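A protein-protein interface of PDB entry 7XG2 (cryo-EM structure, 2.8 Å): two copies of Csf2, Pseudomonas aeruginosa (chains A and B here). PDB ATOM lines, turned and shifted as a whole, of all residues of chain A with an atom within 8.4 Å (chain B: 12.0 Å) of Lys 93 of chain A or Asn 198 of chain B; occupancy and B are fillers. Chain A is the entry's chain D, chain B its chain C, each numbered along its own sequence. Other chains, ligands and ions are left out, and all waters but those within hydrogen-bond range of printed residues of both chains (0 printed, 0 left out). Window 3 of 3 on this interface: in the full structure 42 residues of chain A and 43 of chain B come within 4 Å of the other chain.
N of Asn 198 of chain B sits close to O of Leu 94 of chain A.
The backbone carbonyl oxygen (O) of Val 196 of chain B is in hydrogen-bond range of the backbone NH (N) of Leu 94 of chain A (2.9 Å).
The backbone carbonyl oxygen of Glu 195 of chain B is in hydrogen-bond range of the side-chain amino group of Lys 93 of chain A.
N of Asp 193 of chain B lies within hydrogen-bond range of OG of Ser 190 of chain B (3.1 Å).
OG of Ser 95 of chain A lies within hydrogen-bond range of N of Ala 98 of chain A, 3.0 Å away.
O of Lys 93 of chain A lies close to OG of Ser 335 of chain A, 3.3 Å away.
The side-chain carboxylate (OE2) of Glu 339 of chain A lies within hydrogen-bond range of the backbone NH (N) of Ser 95 of chain A, at 2.5 Å.
Glu 84 of chain A touches Val 196 of chain B (CD to CG1, 3.6 Å).
Val 196 of chain B touches Val 88 of chain A.
Asn 198 of chain B touches Lys 93 of chain A (OD1 to CB, 3.3 Å).
C of Ile 197 of chain B touches O of Leu 94 of chain A, at 3.2 Å.
CD1 of Ile 96 of chain A touches CD1 of Ile 185 of chain B, 3.7 Å away.
CD1 of Ile 96 of chain A touches CG2 of Ile 197 of chain B, at 3.7 Å.
CE3 of Trp 207 of chain B touches CG1 of Ile 96 of chain A (3.6 Å).
Ile 185 of chain B touches Tyr 99 of chain A.
Asp 193 of chain B touches Tyr 99 of chain A.
Tyr 99 of chain A touches Val 196 of chain B.
Of chain B, only Glu 195 (3.0 Å), Val 196 (3.3 Å), Ile 197 (3.5 Å) and Asn 198 (3.3 Å) come within 4 Å of Lys 93 of chain A.
Val 88 of chain A touches two residues of chain B.
No residue of chain B comes within 4 Å of Gly 91 of chain A.
No residue of chain B comes within 4 Å of Asn 92 of chain A.
Ser 95 of chain A touches one residue of chain B.
No residue of chain B comes within 4 Å of Ser 335 of chain A.
Of the printed residues of chain A, Glu 195 of chain B touches Val 88 and Lys 93.
Printed residues of chain A within 4 Å of Asp 193 of chain B: Tyr 99 (3.8 Å).
Printed residues of chain B within 4 Å of Glu 84 of chain A: Val 196 (3.6 Å).
Of the printed residues of chain B, Tyr 99 of chain A touches Ile 185 (3.8 Å), Leu 188 (3.4 Å), Asp 193 (3.8 Å), Val 196 (3.7 Å) and Ile 197 (3.6 Å).
Ser 190 of chain B touches none of the printed residues of chain A.
The nearest residue of chain B that does not touch Lys 93 of chain A is Gly 199 of chain B (5.1 Å).
The nearest residue of chain A that does not touch Asn 198 of chain B is Ser 95 of chain A (4.3 Å).
The nearest printed residue of chain A that does not touch Ala 204 of chain B is Tyr 99 of chain A (8.0 Å).
Printed residues of chain B that touch a printed residue of chain A: Ile 185, Leu 188, Asp 193, Glu 195, Val 196, Ile 197, Asn 198, Ala 203, Ala 204 and Trp 207.
Printed residues of chain A that touch a printed residue of chain B: Glu 84, Val 88, Lys 93, Leu 94, Ser 95, Ile 96 and Tyr 99.
Hydrophobic or aromatic side chains of chain A within 4 Å of the printed part of chain B: Val 88, Leu 94, Ile 96 and Tyr 99.
Among the printed residues, no Asp or Glu carboxylate lies within 4 Å of a Lys or Arg side-chain nitrogen of the other chain.
No position is printed for both chains.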
ATOM      1  N   GLU A  84     -12.126  38.254 -17.309  1.00  0.00           N
ATOM      2  CA  GLU A  84     -11.533  37.081 -17.943  1.00  0.00           C
ATOM      3  C   GLU A  84     -10.092  37.254 -18.435  1.00  0.00           C
ATOM      4  O   GLU A  84      -9.342  36.282 -18.330  1.00  0.00           O
ATOM      5  CB  GLU A  84     -12.418  36.580 -19.088  1.00  0.00           C
ATOM      6  CG  GLU A  84     -13.556  35.694 -18.631  1.00  0.00           C
ATOM      7  CD  GLU A  84     -14.357  35.141 -19.788  1.00  0.00           C
ATOM      8  OE1 GLU A  84     -13.765  34.880 -20.855  1.00  0.00           O
ATOM      9  OE2 GLU A  84     -15.578  34.958 -19.629  1.00  0.00           O
ATOM     10  N   LEU A  87      -8.162  36.837 -15.388  1.00  0.00           N
ATOM     11  CA  LEU A  87      -8.376  35.514 -14.826  1.00  0.00           C
ATOM     12  C   LEU A  87      -7.695  34.414 -15.633  1.00  0.00           C
ATOM     13  O   LEU A  87      -7.417  33.342 -15.085  1.00  0.00           O
ATOM     14  CB  LEU A  87      -9.879  35.254 -14.736  1.00  0.00           C
ATOM     15  CG  LEU A  87     -10.448  34.451 -13.577  1.00  0.00           C
ATOM     16  CD1 LEU A  87      -9.965  35.021 -12.262  1.00  0.00           C
ATOM     17  CD2 LEU A  87     -11.942  34.568 -13.660  1.00  0.00           C
ATOM     18  N   VAL A  88      -7.432  34.658 -16.917  1.00  0.00           N
ATOM     19  CA  VAL A  88      -6.616  33.770 -17.741  1.00  0.00           C
ATOM     20  C   VAL A  88      -5.122  34.082 -17.639  1.00  0.00           C
ATOM     21  O   VAL A  88      -4.305  33.148 -17.679  1.00  0.00           O
ATOM     22  CB  VAL A  88      -7.101  33.811 -19.211  1.00  0.00           C
ATOM     23  CG1 VAL A  88      -6.285  32.911 -20.113  1.00  0.00           C
ATOM     24  CG2 VAL A  88      -8.529  33.321 -19.285  1.00  0.00           C
ATOM     25  N   GLU A  89      -4.741  35.349 -17.434  1.00  0.00           N
ATOM     26  CA  GLU A  89      -3.319  35.675 -17.332  1.00  0.00           C
ATOM     27  C   GLU A  89      -2.672  35.116 -16.065  1.00  0.00           C
ATOM     28  O   GLU A  89      -1.440  35.060 -15.989  1.00  0.00           O
ATOM     29  CB  GLU A  89      -3.102  37.187 -17.411  1.00  0.00           C
ATOM     30  CG  GLU A  89      -3.267  37.933 -16.103  1.00  0.00           C
ATOM     31  CD  GLU A  89      -2.937  39.403 -16.241  1.00  0.00           C
ATOM     32  OE1 GLU A  89      -2.788  39.871 -17.390  1.00  0.00           O
ATOM     33  OE2 GLU A  89      -2.815  40.088 -15.204  1.00  0.00           O
ATOM     34  N   LYS A  90      -3.464  34.704 -15.082  1.00  0.00           N
ATOM     35  CA  LYS A  90      -3.003  33.840 -14.008  1.00  0.00           C
ATOM     36  C   LYS A  90      -3.673  32.473 -14.130  1.00  0.00           C
ATOM     37  O   LYS A  90      -4.516  32.239 -14.996  1.00  0.00           O
ATOM     38  CB  LYS A  90      -3.284  34.474 -12.645  1.00  0.00           C
ATOM     39  CG  LYS A  90      -2.560  35.796 -12.437  1.00  0.00           C
ATOM     40  CD  LYS A  90      -2.773  36.333 -11.035  1.00  0.00           C
ATOM     41  CE  LYS A  90      -4.237  36.635 -10.774  1.00  0.00           C
ATOM     42  NZ  LYS A  90      -4.459  37.077  -9.372  1.00  0.00           N
ATOM     43  N   GLY A  91      -3.310  31.568 -13.227  1.00  0.00           N
ATOM     44  CA  GLY A  91      -3.740  30.186 -13.361  1.00  0.00           C
ATOM     45  C   GLY A  91      -5.167  29.888 -12.947  1.00  0.00           C
ATOM     46  O   GLY A  91      -5.537  28.712 -12.884  1.00  0.00           O
ATOM     47  N   ASN A  92      -5.973  30.908 -12.658  1.00  0.00           N
ATOM     48  CA  ASN A  92      -7.330  30.691 -12.180  1.00  0.00           C
ATOM     49  C   ASN A  92      -8.238  30.211 -13.308  1.00  0.00           C
ATOM     50  O   ASN A  92      -8.054  30.553 -14.477  1.00  0.00           O
ATOM     51  CB  ASN A  92      -7.881  31.979 -11.574  1.00  0.00           C
ATOM     52  CG  ASN A  92      -6.821  32.772 -10.838  1.00  0.00           C
ATOM     53  OD1 ASN A  92      -6.494  33.896 -11.218  1.00  0.00           O
ATOM     54  ND2 ASN A  92      -6.281  32.192  -9.774  1.00  0.00           N
ATOM     55  N   LYS A  93      -9.229  29.403 -12.938  1.00  0.00           N
ATOM     56  CA  LYS A  93     -10.189  28.875 -13.892  1.00  0.00           C
ATOM     57  C   LYS A  93     -11.511  28.639 -13.176  1.00  0.00           C
ATOM     58  O   LYS A  93     -11.548  28.348 -11.978  1.00  0.00           O
ATOM     59  CB  LYS A  93      -9.680  27.582 -14.542  1.00  0.00           C
ATOM     60  CG  LYS A  93     -10.165  27.368 -15.964  1.00  0.00           C
ATOM     61  CD  LYS A  93      -9.287  26.389 -16.725  1.00  0.00           C
ATOM     62  CE  LYS A  93      -7.889  26.944 -16.934  1.00  0.00           C
ATOM     63  NZ  LYS A  93      -7.918  28.360 -17.394  1.00  0.00           N
ATOM     64  N   LEU A  94     -12.598  28.755 -13.929  1.00  0.00           N
ATOM     65  CA  LEU A  94     -13.950  28.697 -13.394  1.00  0.00           C
ATOM     66  C   LEU A  94     -14.594  27.368 -13.750  1.00  0.00           C
ATOM     67  O   LEU A  94     -14.254  26.762 -14.765  1.00  0.00           O
ATOM     68  CB  LEU A  94     -14.802  29.842 -13.953  1.00  0.00           C
ATOM     69  CG  LEU A  94     -15.067  31.064 -13.077  1.00  0.00           C
ATOM     70  CD1 LEU A  94     -13.785  31.617 -12.517  1.00  0.00           C
ATOM     71  CD2 LEU A  94     -15.807  32.125 -13.875  1.00  0.00           C
ATOM     72  N   SER A  95     -15.523  26.911 -12.919  1.00  0.00           N
ATOM     73  CA  SER A  95     -16.363  25.803 -13.341  1.00  0.00           C
ATOM     74  C   SER A  95     -17.424  26.313 -14.310  1.00  0.00           C
ATOM     75  O   SER A  95     -17.595  27.520 -14.502  1.00  0.00           O
ATOM     76  CB  SER A  95     -17.010  25.115 -12.140  1.00  0.00           C
ATOM     77  OG  SER A  95     -17.991  25.935 -11.535  1.00  0.00           O
ATOM     78  N   ILE A  96     -18.131  25.374 -14.945  1.00  0.00           N
ATOM     79  CA  ILE A  96     -19.156  25.758 -15.912  1.00  0.00           C
ATOM     80  C   ILE A  96     -20.343  26.410 -15.202  1.00  0.00           C
ATOM     81  O   ILE A  96     -20.961  27.348 -15.725  1.00  0.00           O
ATOM     82  CB  ILE A  96     -19.553  24.545 -16.787  1.00  0.00           C
ATOM     83  CG1 ILE A  96     -20.296  24.994 -18.046  1.00  0.00           C
ATOM     84  CG2 ILE A  96     -20.312  23.457 -16.017  1.00  0.00           C
ATOM     85  CD1 ILE A  96     -19.401  25.208 -19.234  1.00  0.00           C
ATOM     86  N   GLY A  97     -20.627  25.980 -13.969  1.00  0.00           N
ATOM     87  CA  GLY A  97     -21.612  26.670 -13.160  1.00  0.00           C
ATOM     88  C   GLY A  97     -21.123  28.014 -12.669  1.00  0.00           C
ATOM     89  O   GLY A  97     -21.920  28.934 -12.487  1.00  0.00           O
ATOM     90  N   ALA A  98     -19.810  28.163 -12.487  1.00  0.00           N
ATOM     91  CA  ALA A  98     -19.268  29.451 -12.069  1.00  0.00           C
ATOM     92  C   ALA A  98     -19.263  30.451 -13.216  1.00  0.00           C
ATOM     93  O   ALA A  98     -19.514  31.641 -13.005  1.00  0.00           O
ATOM     94  CB  ALA A  98     -17.867  29.269 -11.494  1.00  0.00           C
ATOM     95  N   TYR A  99     -18.985  29.981 -14.435  1.00  0.00           N
ATOM     96  CA  TYR A  99     -19.132  30.813 -15.625  1.00  0.00           C
ATOM     97  C   TYR A  99     -20.588  31.217 -15.824  1.00  0.00           C
ATOM     98  O   TYR A  99     -20.892  32.380 -16.133  1.00  0.00           O
ATOM     99  CB  TYR A  99     -18.605  30.046 -16.840  1.00  0.00           C
ATOM    100  CG  TYR A  99     -18.517  30.829 -18.130  1.00  0.00           C
ATOM    101  CD1 TYR A  99     -17.355  31.505 -18.467  1.00  0.00           C
ATOM    102  CD2 TYR A  99     -19.579  30.858 -19.029  1.00  0.00           C
ATOM    103  CE1 TYR A  99     -17.256  32.204 -19.648  1.00  0.00           C
ATOM    104  CE2 TYR A  99     -19.492  31.565 -20.210  1.00  0.00           C
ATOM    105  CZ  TYR A  99     -18.327  32.238 -20.512  1.00  0.00           C
ATOM    106  OH  TYR A  99     -18.227  32.942 -21.689  1.00  0.00           O
ATOM    107  N   SER A 334      -9.259  36.263  -8.184  1.00  0.00           N
ATOM    108  CA  SER A 334      -9.051  34.826  -8.254  1.00  0.00           C
ATOM    109  C   SER A 334     -10.397  34.151  -8.459  1.00  0.00           C
ATOM    110  O   SER A 334     -11.452  34.788  -8.404  1.00  0.00           O
ATOM    111  CB  SER A 334      -8.363  34.293  -6.996  1.00  0.00           C
ATOM    112  OG  SER A 334      -8.469  32.882  -6.930  1.00  0.00           O
ATOM    113  N   SER A 335     -10.349  32.846  -8.697  1.00  0.00           N
ATOM    114  CA  SER A 335     -11.543  32.071  -8.993  1.00  0.00           C
ATOM    115  C   SER A 335     -12.230  31.526  -7.751  1.00  0.00           C
ATOM    116  O   SER A 335     -13.320  30.958  -7.874  1.00  0.00           O
ATOM    117  CB  SER A 335     -11.194  30.910  -9.927  1.00  0.00           C
ATOM    118  OG  SER A 335     -10.514  29.884  -9.227  1.00  0.00           O
ATOM    119  N   LYS A 336     -11.622  31.682  -6.572  1.00  0.00           N
ATOM    120  CA  LYS A 336     -12.175  31.101  -5.350  1.00  0.00           C
ATOM    121  C   LYS A 336     -13.492  31.765  -4.964  1.00  0.00           C
ATOM    122  O   LYS A 336     -14.450  31.084  -4.576  1.00  0.00           O
ATOM    123  CB  LYS A 336     -11.160  31.211  -4.210  1.00  0.00           C
ATOM    124  CG  LYS A 336     -10.347  32.497  -4.218  1.00  0.00           C
ATOM    125  CD  LYS A 336      -9.110  32.383  -3.342  1.00  0.00           C
ATOM    126  CE  LYS A 336      -8.092  31.427  -3.939  1.00  0.00           C
ATOM    127  NZ  LYS A 336      -6.852  31.352  -3.118  1.00  0.00           N
ATOM    128  N   PHE A 338     -15.537  33.325  -7.053  1.00  0.00           N
ATOM    129  CA  PHE A 338     -16.517  32.932  -8.063  1.00  0.00           C
ATOM    130  C   PHE A 338     -17.053  31.529  -7.801  1.00  0.00           C
ATOM    131  O   PHE A 338     -18.259  31.276  -7.944  1.00  0.00           O
ATOM    132  CB  PHE A 338     -15.888  33.011  -9.452  1.00  0.00           C
ATOM    133  CG  PHE A 338     -15.826  34.400 -10.008  1.00  0.00           C
ATOM    134  CD1 PHE A 338     -16.908  34.938 -10.683  1.00  0.00           C
ATOM    135  CD2 PHE A 338     -14.684  35.168  -9.858  1.00  0.00           C
ATOM    136  CE1 PHE A 338     -16.854  36.218 -11.195  1.00  0.00           C
ATOM    137  CE2 PHE A 338     -14.622  36.450 -10.368  1.00  0.00           C
ATOM    138  CZ  PHE A 338     -15.710  36.975 -11.038  1.00  0.00           C
ATOM    139  N   GLU A 339     -16.172  30.610  -7.391  1.00  0.00           N
ATOM    140  CA  GLU A 339     -16.597  29.240  -7.122  1.00  0.00           C
ATOM    141  C   GLU A 339     -17.476  29.157  -5.881  1.00  0.00           C
ATOM    142  O   GLU A 339     -18.484  28.441  -5.880  1.00  0.00           O
ATOM    143  CB  GLU A 339     -15.380  28.325  -6.976  1.00  0.00           C
ATOM    144  CG  GLU A 339     -14.663  28.023  -8.282  1.00  0.00           C
ATOM    145  CD  GLU A 339     -15.493  27.211  -9.256  1.00  0.00           C
ATOM    146  OE1 GLU A 339     -16.369  26.436  -8.815  1.00  0.00           O
ATOM    147  OE2 GLU A 339     -15.268  27.361 -10.473  1.00  0.00           O
ATOM    148  N   ILE B 185     -23.807  29.576 -21.904  1.00  0.00           N
ATOM    149  CA  ILE B 185     -23.088  28.480 -22.535  1.00  0.00           C
ATOM    150  C   ILE B 185     -23.500  28.359 -23.996  1.00  0.00           C
ATOM    151  O   ILE B 185     -22.703  27.956 -24.850  1.00  0.00           O
ATOM    152  CB  ILE B 185     -23.325  27.177 -21.751  1.00  0.00           C
ATOM    153  CG1 ILE B 185     -23.196  27.423 -20.243  1.00  0.00           C
ATOM    154  CG2 ILE B 185     -22.345  26.096 -22.173  1.00  0.00           C
ATOM    155  CD1 ILE B 185     -21.838  27.949 -19.794  1.00  0.00           C
ATOM    156  N   LEU B 188     -21.358  30.702 -25.949  1.00  0.00           N
ATOM    157  CA  LEU B 188     -19.948  30.376 -26.115  1.00  0.00           C
ATOM    158  C   LEU B 188     -19.676  30.048 -27.578  1.00  0.00           C
ATOM    159  O   LEU B 188     -20.388  29.242 -28.184  1.00  0.00           O
ATOM    160  CB  LEU B 188     -19.562  29.200 -25.224  1.00  0.00           C
ATOM    161  CG  LEU B 188     -19.267  29.532 -23.765  1.00  0.00           C
ATOM    162  CD1 LEU B 188     -19.350  28.283 -22.914  1.00  0.00           C
ATOM    163  CD2 LEU B 188     -17.901  30.178 -23.640  1.00  0.00           C
ATOM    164  N   SER B 190     -16.082  30.207 -29.182  1.00  0.00           N
ATOM    165  CA  SER B 190     -14.711  29.974 -29.610  1.00  0.00           C
ATOM    166  C   SER B 190     -13.934  29.338 -28.468  1.00  0.00           C
ATOM    167  O   SER B 190     -14.410  29.258 -27.334  1.00  0.00           O
ATOM    168  CB  SER B 190     -14.046  31.273 -30.072  1.00  0.00           C
ATOM    169  OG  SER B 190     -13.814  32.143 -28.981  1.00  0.00           O
ATOM    170  N   SER B 191     -12.728  28.868 -28.796  1.00  0.00           N
ATOM    171  CA  SER B 191     -11.857  28.272 -27.788  1.00  0.00           C
ATOM    172  C   SER B 191     -11.384  29.311 -26.781  1.00  0.00           C
ATOM    173  O   SER B 191     -11.277  29.021 -25.583  1.00  0.00           O
ATOM    174  CB  SER B 191     -10.665  27.594 -28.460  1.00  0.00           C
ATOM    175  OG  SER B 191      -9.712  28.552 -28.883  1.00  0.00           O
ATOM    176  N   GLU B 192     -11.106  30.533 -27.248  1.00  0.00           N
ATOM    177  CA  GLU B 192     -10.714  31.606 -26.340  1.00  0.00           C
ATOM    178  C   GLU B 192     -11.889  32.073 -25.493  1.00  0.00           C
ATOM    179  O   GLU B 192     -11.691  32.663 -24.426  1.00  0.00           O
ATOM    180  CB  GLU B 192     -10.117  32.792 -27.110  1.00  0.00           C
ATOM    181  CG  GLU B 192     -10.671  33.065 -28.518  1.00  0.00           C
ATOM    182  CD  GLU B 192     -10.014  32.249 -29.630  1.00  0.00           C
ATOM    183  OE1 GLU B 192      -9.538  31.124 -29.370  1.00  0.00           O
ATOM    184  OE2 GLU B 192      -9.983  32.743 -30.777  1.00  0.00           O
ATOM    185  N   ASP B 193     -13.114  31.824 -25.956  1.00  0.00           N
ATOM    186  CA  ASP B 193     -14.291  32.124 -25.151  1.00  0.00           C
ATOM    187  C   ASP B 193     -14.424  31.149 -23.987  1.00  0.00           C
ATOM    188  O   ASP B 193     -14.915  31.514 -22.914  1.00  0.00           O
ATOM    189  CB  ASP B 193     -15.541  32.074 -26.029  1.00  0.00           C
ATOM    190  CG  ASP B 193     -16.100  33.445 -26.330  1.00  0.00           C
ATOM    191  OD1 ASP B 193     -15.511  34.445 -25.867  1.00  0.00           O
ATOM    192  OD2 ASP B 193     -17.128  33.527 -27.031  1.00  0.00           O
ATOM    193  N   VAL B 194     -13.972  29.907 -24.177  1.00  0.00           N
ATOM    194  CA  VAL B 194     -14.293  28.822 -23.258  1.00  0.00           C
ATOM    195  C   VAL B 194     -13.095  28.411 -22.408  1.00  0.00           C
ATOM    196  O   VAL B 194     -13.258  27.649 -21.447  1.00  0.00           O
ATOM    197  CB  VAL B 194     -14.833  27.607 -24.043  1.00  0.00           C
ATOM    198  CG1 VAL B 194     -13.696  26.866 -24.748  1.00  0.00           C
ATOM    199  CG2 VAL B 194     -15.746  26.700 -23.204  1.00  0.00           C
ATOM    200  N   GLU B 195     -11.896  28.908 -22.710  1.00  0.00           N
ATOM    201  CA  GLU B 195     -10.717  28.449 -21.985  1.00  0.00           C
ATOM    202  C   GLU B 195     -10.588  29.043 -20.585  1.00  0.00           C
ATOM    203  O   GLU B 195      -9.650  28.685 -19.865  1.00  0.00           O
ATOM    204  CB  GLU B 195      -9.449  28.742 -22.788  1.00  0.00           C
ATOM    205  CG  GLU B 195      -9.317  30.165 -23.248  1.00  0.00           C
ATOM    206  CD  GLU B 195      -8.457  30.979 -22.333  1.00  0.00           C
ATOM    207  OE1 GLU B 195      -7.760  30.365 -21.499  1.00  0.00           O
ATOM    208  OE2 GLU B 195      -8.478  32.220 -22.456  1.00  0.00           O
ATOM    209  N   VAL B 196     -11.497  29.939 -20.182  1.00  0.00           N
ATOM    210  CA  VAL B 196     -11.605  30.352 -18.784  1.00  0.00           C
ATOM    211  C   VAL B 196     -12.424  29.366 -17.964  1.00  0.00           C
ATOM    212  O   VAL B 196     -12.533  29.516 -16.740  1.00  0.00           O
ATOM    213  CB  VAL B 196     -12.193  31.779 -18.732  1.00  0.00           C
ATOM    214  CG1 VAL B 196     -13.712  31.751 -18.848  1.00  0.00           C
ATOM    215  CG2 VAL B 196     -11.723  32.547 -17.488  1.00  0.00           C
ATOM    216  N   ILE B 197     -12.978  28.336 -18.596  1.00  0.00           N
ATOM    217  CA  ILE B 197     -13.818  27.345 -17.934  1.00  0.00           C
ATOM    218  C   ILE B 197     -12.988  26.094 -17.682  1.00  0.00           C
ATOM    219  O   ILE B 197     -12.210  25.676 -18.550  1.00  0.00           O
ATOM    220  CB  ILE B 197     -15.065  27.021 -18.772  1.00  0.00           C
ATOM    221  CG1 ILE B 197     -15.716  28.315 -19.263  1.00  0.00           C
ATOM    222  CG2 ILE B 197     -16.045  26.193 -17.969  1.00  0.00           C
ATOM    223  CD1 ILE B 197     -17.051  28.121 -19.943  1.00  0.00           C
ATOM    224  N   ASN B 198     -13.120  25.526 -16.479  1.00  0.00           N
ATOM    225  CA  ASN B 198     -12.538  24.221 -16.182  1.00  0.00           C
ATOM    226  C   ASN B 198     -13.146  23.162 -17.089  1.00  0.00           C
ATOM    227  O   ASN B 198     -14.369  23.067 -17.221  1.00  0.00           O
ATOM    228  CB  ASN B 198     -12.773  23.849 -14.718  1.00  0.00           C
ATOM    229  CG  ASN B 198     -11.612  24.225 -13.827  1.00  0.00           C
ATOM    230  OD1 ASN B 198     -10.480  24.355 -14.289  1.00  0.00           O
ATOM    231  ND2 ASN B 198     -11.888  24.406 -12.541  1.00  0.00           N
ATOM    232  N   GLY B 199     -12.285  22.367 -17.718  1.00  0.00           N
ATOM    233  CA  GLY B 199     -12.686  21.487 -18.786  1.00  0.00           C
ATOM    234  C   GLY B 199     -12.722  22.140 -20.151  1.00  0.00           C
ATOM    235  O   GLY B 199     -12.223  21.554 -21.117  1.00  0.00           O
ATOM    236  N   GLY B 200     -13.276  23.344 -20.253  1.00  0.00           N
ATOM    237  CA  GLY B 200     -13.308  24.036 -21.523  1.00  0.00           C
ATOM    238  C   GLY B 200     -14.373  23.478 -22.435  1.00  0.00           C
ATOM    239  O   GLY B 200     -15.573  23.518 -22.128  1.00  0.00           O
ATOM    240  N   ALA B 201     -13.928  22.940 -23.574  1.00  0.00           N
ATOM    241  CA  ALA B 201     -14.849  22.474 -24.604  1.00  0.00           C
ATOM    242  C   ALA B 201     -15.637  21.249 -24.160  1.00  0.00           C
ATOM    243  O   ALA B 201     -16.817  21.125 -24.502  1.00  0.00           O
ATOM    244  CB  ALA B 201     -14.083  22.173 -25.892  1.00  0.00           C
ATOM    245  N   VAL B 202     -15.018  20.350 -23.392  1.00  0.00           N
ATOM    246  CA  VAL B 202     -15.709  19.132 -22.969  1.00  0.00           C
ATOM    247  C   VAL B 202     -16.794  19.455 -21.940  1.00  0.00           C
ATOM    248  O   VAL B 202     -17.909  18.923 -22.008  1.00  0.00           O
ATOM    249  CB  VAL B 202     -14.696  18.080 -22.466  1.00  0.00           C
ATOM    250  CG1 VAL B 202     -13.758  18.634 -21.395  1.00  0.00           C
ATOM    251  CG2 VAL B 202     -15.404  16.824 -21.971  1.00  0.00           C
ATOM    252  N   ALA B 203     -16.515  20.383 -21.018  1.00  0.00           N
ATOM    253  CA  ALA B 203     -17.526  20.788 -20.043  1.00  0.00           C
ATOM    254  C   ALA B 203     -18.626  21.611 -20.699  1.00  0.00           C
ATOM    255  O   ALA B 203     -19.803  21.494 -20.329  1.00  0.00           O
ATOM    256  CB  ALA B 203     -16.877  21.569 -18.903  1.00  0.00           C
ATOM    257  N   ALA B 204     -18.258  22.437 -21.685  1.00  0.00           N
ATOM    258  CA  ALA B 204     -19.250  23.197 -22.439  1.00  0.00           C
ATOM    259  C   ALA B 204     -20.183  22.275 -23.213  1.00  0.00           C
ATOM    260  O   ALA B 204     -21.405  22.438 -23.166  1.00  0.00           O
ATOM    261  CB  ALA B 204     -18.552  24.175 -23.382  1.00  0.00           C
ATOM    262  N   ASN B 205     -19.622  21.264 -23.886  1.00  0.00           N
ATOM    263  CA  ASN B 205     -20.440  20.312 -24.634  1.00  0.00           C
ATOM    264  C   ASN B 205     -21.271  19.440 -23.705  1.00  0.00           C
ATOM    265  O   ASN B 205     -22.377  19.020 -24.067  1.00  0.00           O
ATOM    266  CB  ASN B 205     -19.556  19.445 -25.528  1.00  0.00           C
ATOM    267  CG  ASN B 205     -19.052  20.188 -26.747  1.00  0.00           C
ATOM    268  OD1 ASN B 205     -19.677  20.156 -27.804  1.00  0.00           O
ATOM    269  ND2 ASN B 205     -17.915  20.855 -26.607  1.00  0.00           N
ATOM    270  N   GLY B 206     -20.759  19.160 -22.503  1.00  0.00           N
ATOM    271  CA  GLY B 206     -21.566  18.472 -21.509  1.00  0.00           C
ATOM    272  C   GLY B 206     -22.759  19.294 -21.060  1.00  0.00           C
ATOM    273  O   GLY B 206     -23.855  18.760 -20.875  1.00  0.00           O
ATOM    274  N   TRP B 207     -22.560  20.608 -20.899  1.00  0.00           N
ATOM    275  CA  TRP B 207     -23.675  21.503 -20.592  1.00  0.00           C
ATOM    276  C   TRP B 207     -24.688  21.537 -21.730  1.00  0.00           C
ATOM    277  O   TRP B 207     -25.901  21.541 -21.484  1.00  0.00           O
ATOM    278  CB  TRP B 207     -23.157  22.912 -20.292  1.00  0.00           C
ATOM    279  CG  TRP B 207     -24.214  23.894 -19.809  1.00  0.00           C
ATOM    280  CD1 TRP B 207     -25.213  24.479 -20.545  1.00  0.00           C
ATOM    281  CD2 TRP B 207     -24.361  24.395 -18.480  1.00  0.00           C
ATOM    282  NE1 TRP B 207     -25.964  25.306 -19.754  1.00  0.00           N
ATOM    283  CE2 TRP B 207     -25.461  25.274 -18.481  1.00  0.00           C
ATOM    284  CE3 TRP B 207     -23.671  24.184 -17.285  1.00  0.00           C
ATOM    285  CZ2 TRP B 207     -25.879  25.940 -17.341  1.00  0.00           C
ATOM    286  CZ3 TRP B 207     -24.085  24.848 -16.158  1.00  0.00           C
ATOM    287  CH2 TRP B 207     -25.177  25.714 -16.192  1.00  0.00           C
ATOM    288  N   ILE B 208     -24.206  21.588 -22.979  1.00  0.00           N
ATOM    289  CA  ILE B 208     -25.109  21.613 -24.133  1.00  0.00           C
ATOM    290  C   ILE B 208     -25.927  20.329 -24.198  1.00  0.00           C
ATOM    291  O   ILE B 208     -27.147  20.366 -24.388  1.00  0.00           O
ATOM    292  CB  ILE B 208     -24.340  21.840 -25.450  1.00  0.00           C
ATOM    293  CG1 ILE B 208     -23.509  23.118 -25.422  1.00  0.00           C
ATOM    294  CG2 ILE B 208     -25.308  21.910 -26.619  1.00  0.00           C
ATOM    295  CD1 ILE B 208     -24.282  24.348 -25.164  1.00  0.00           C
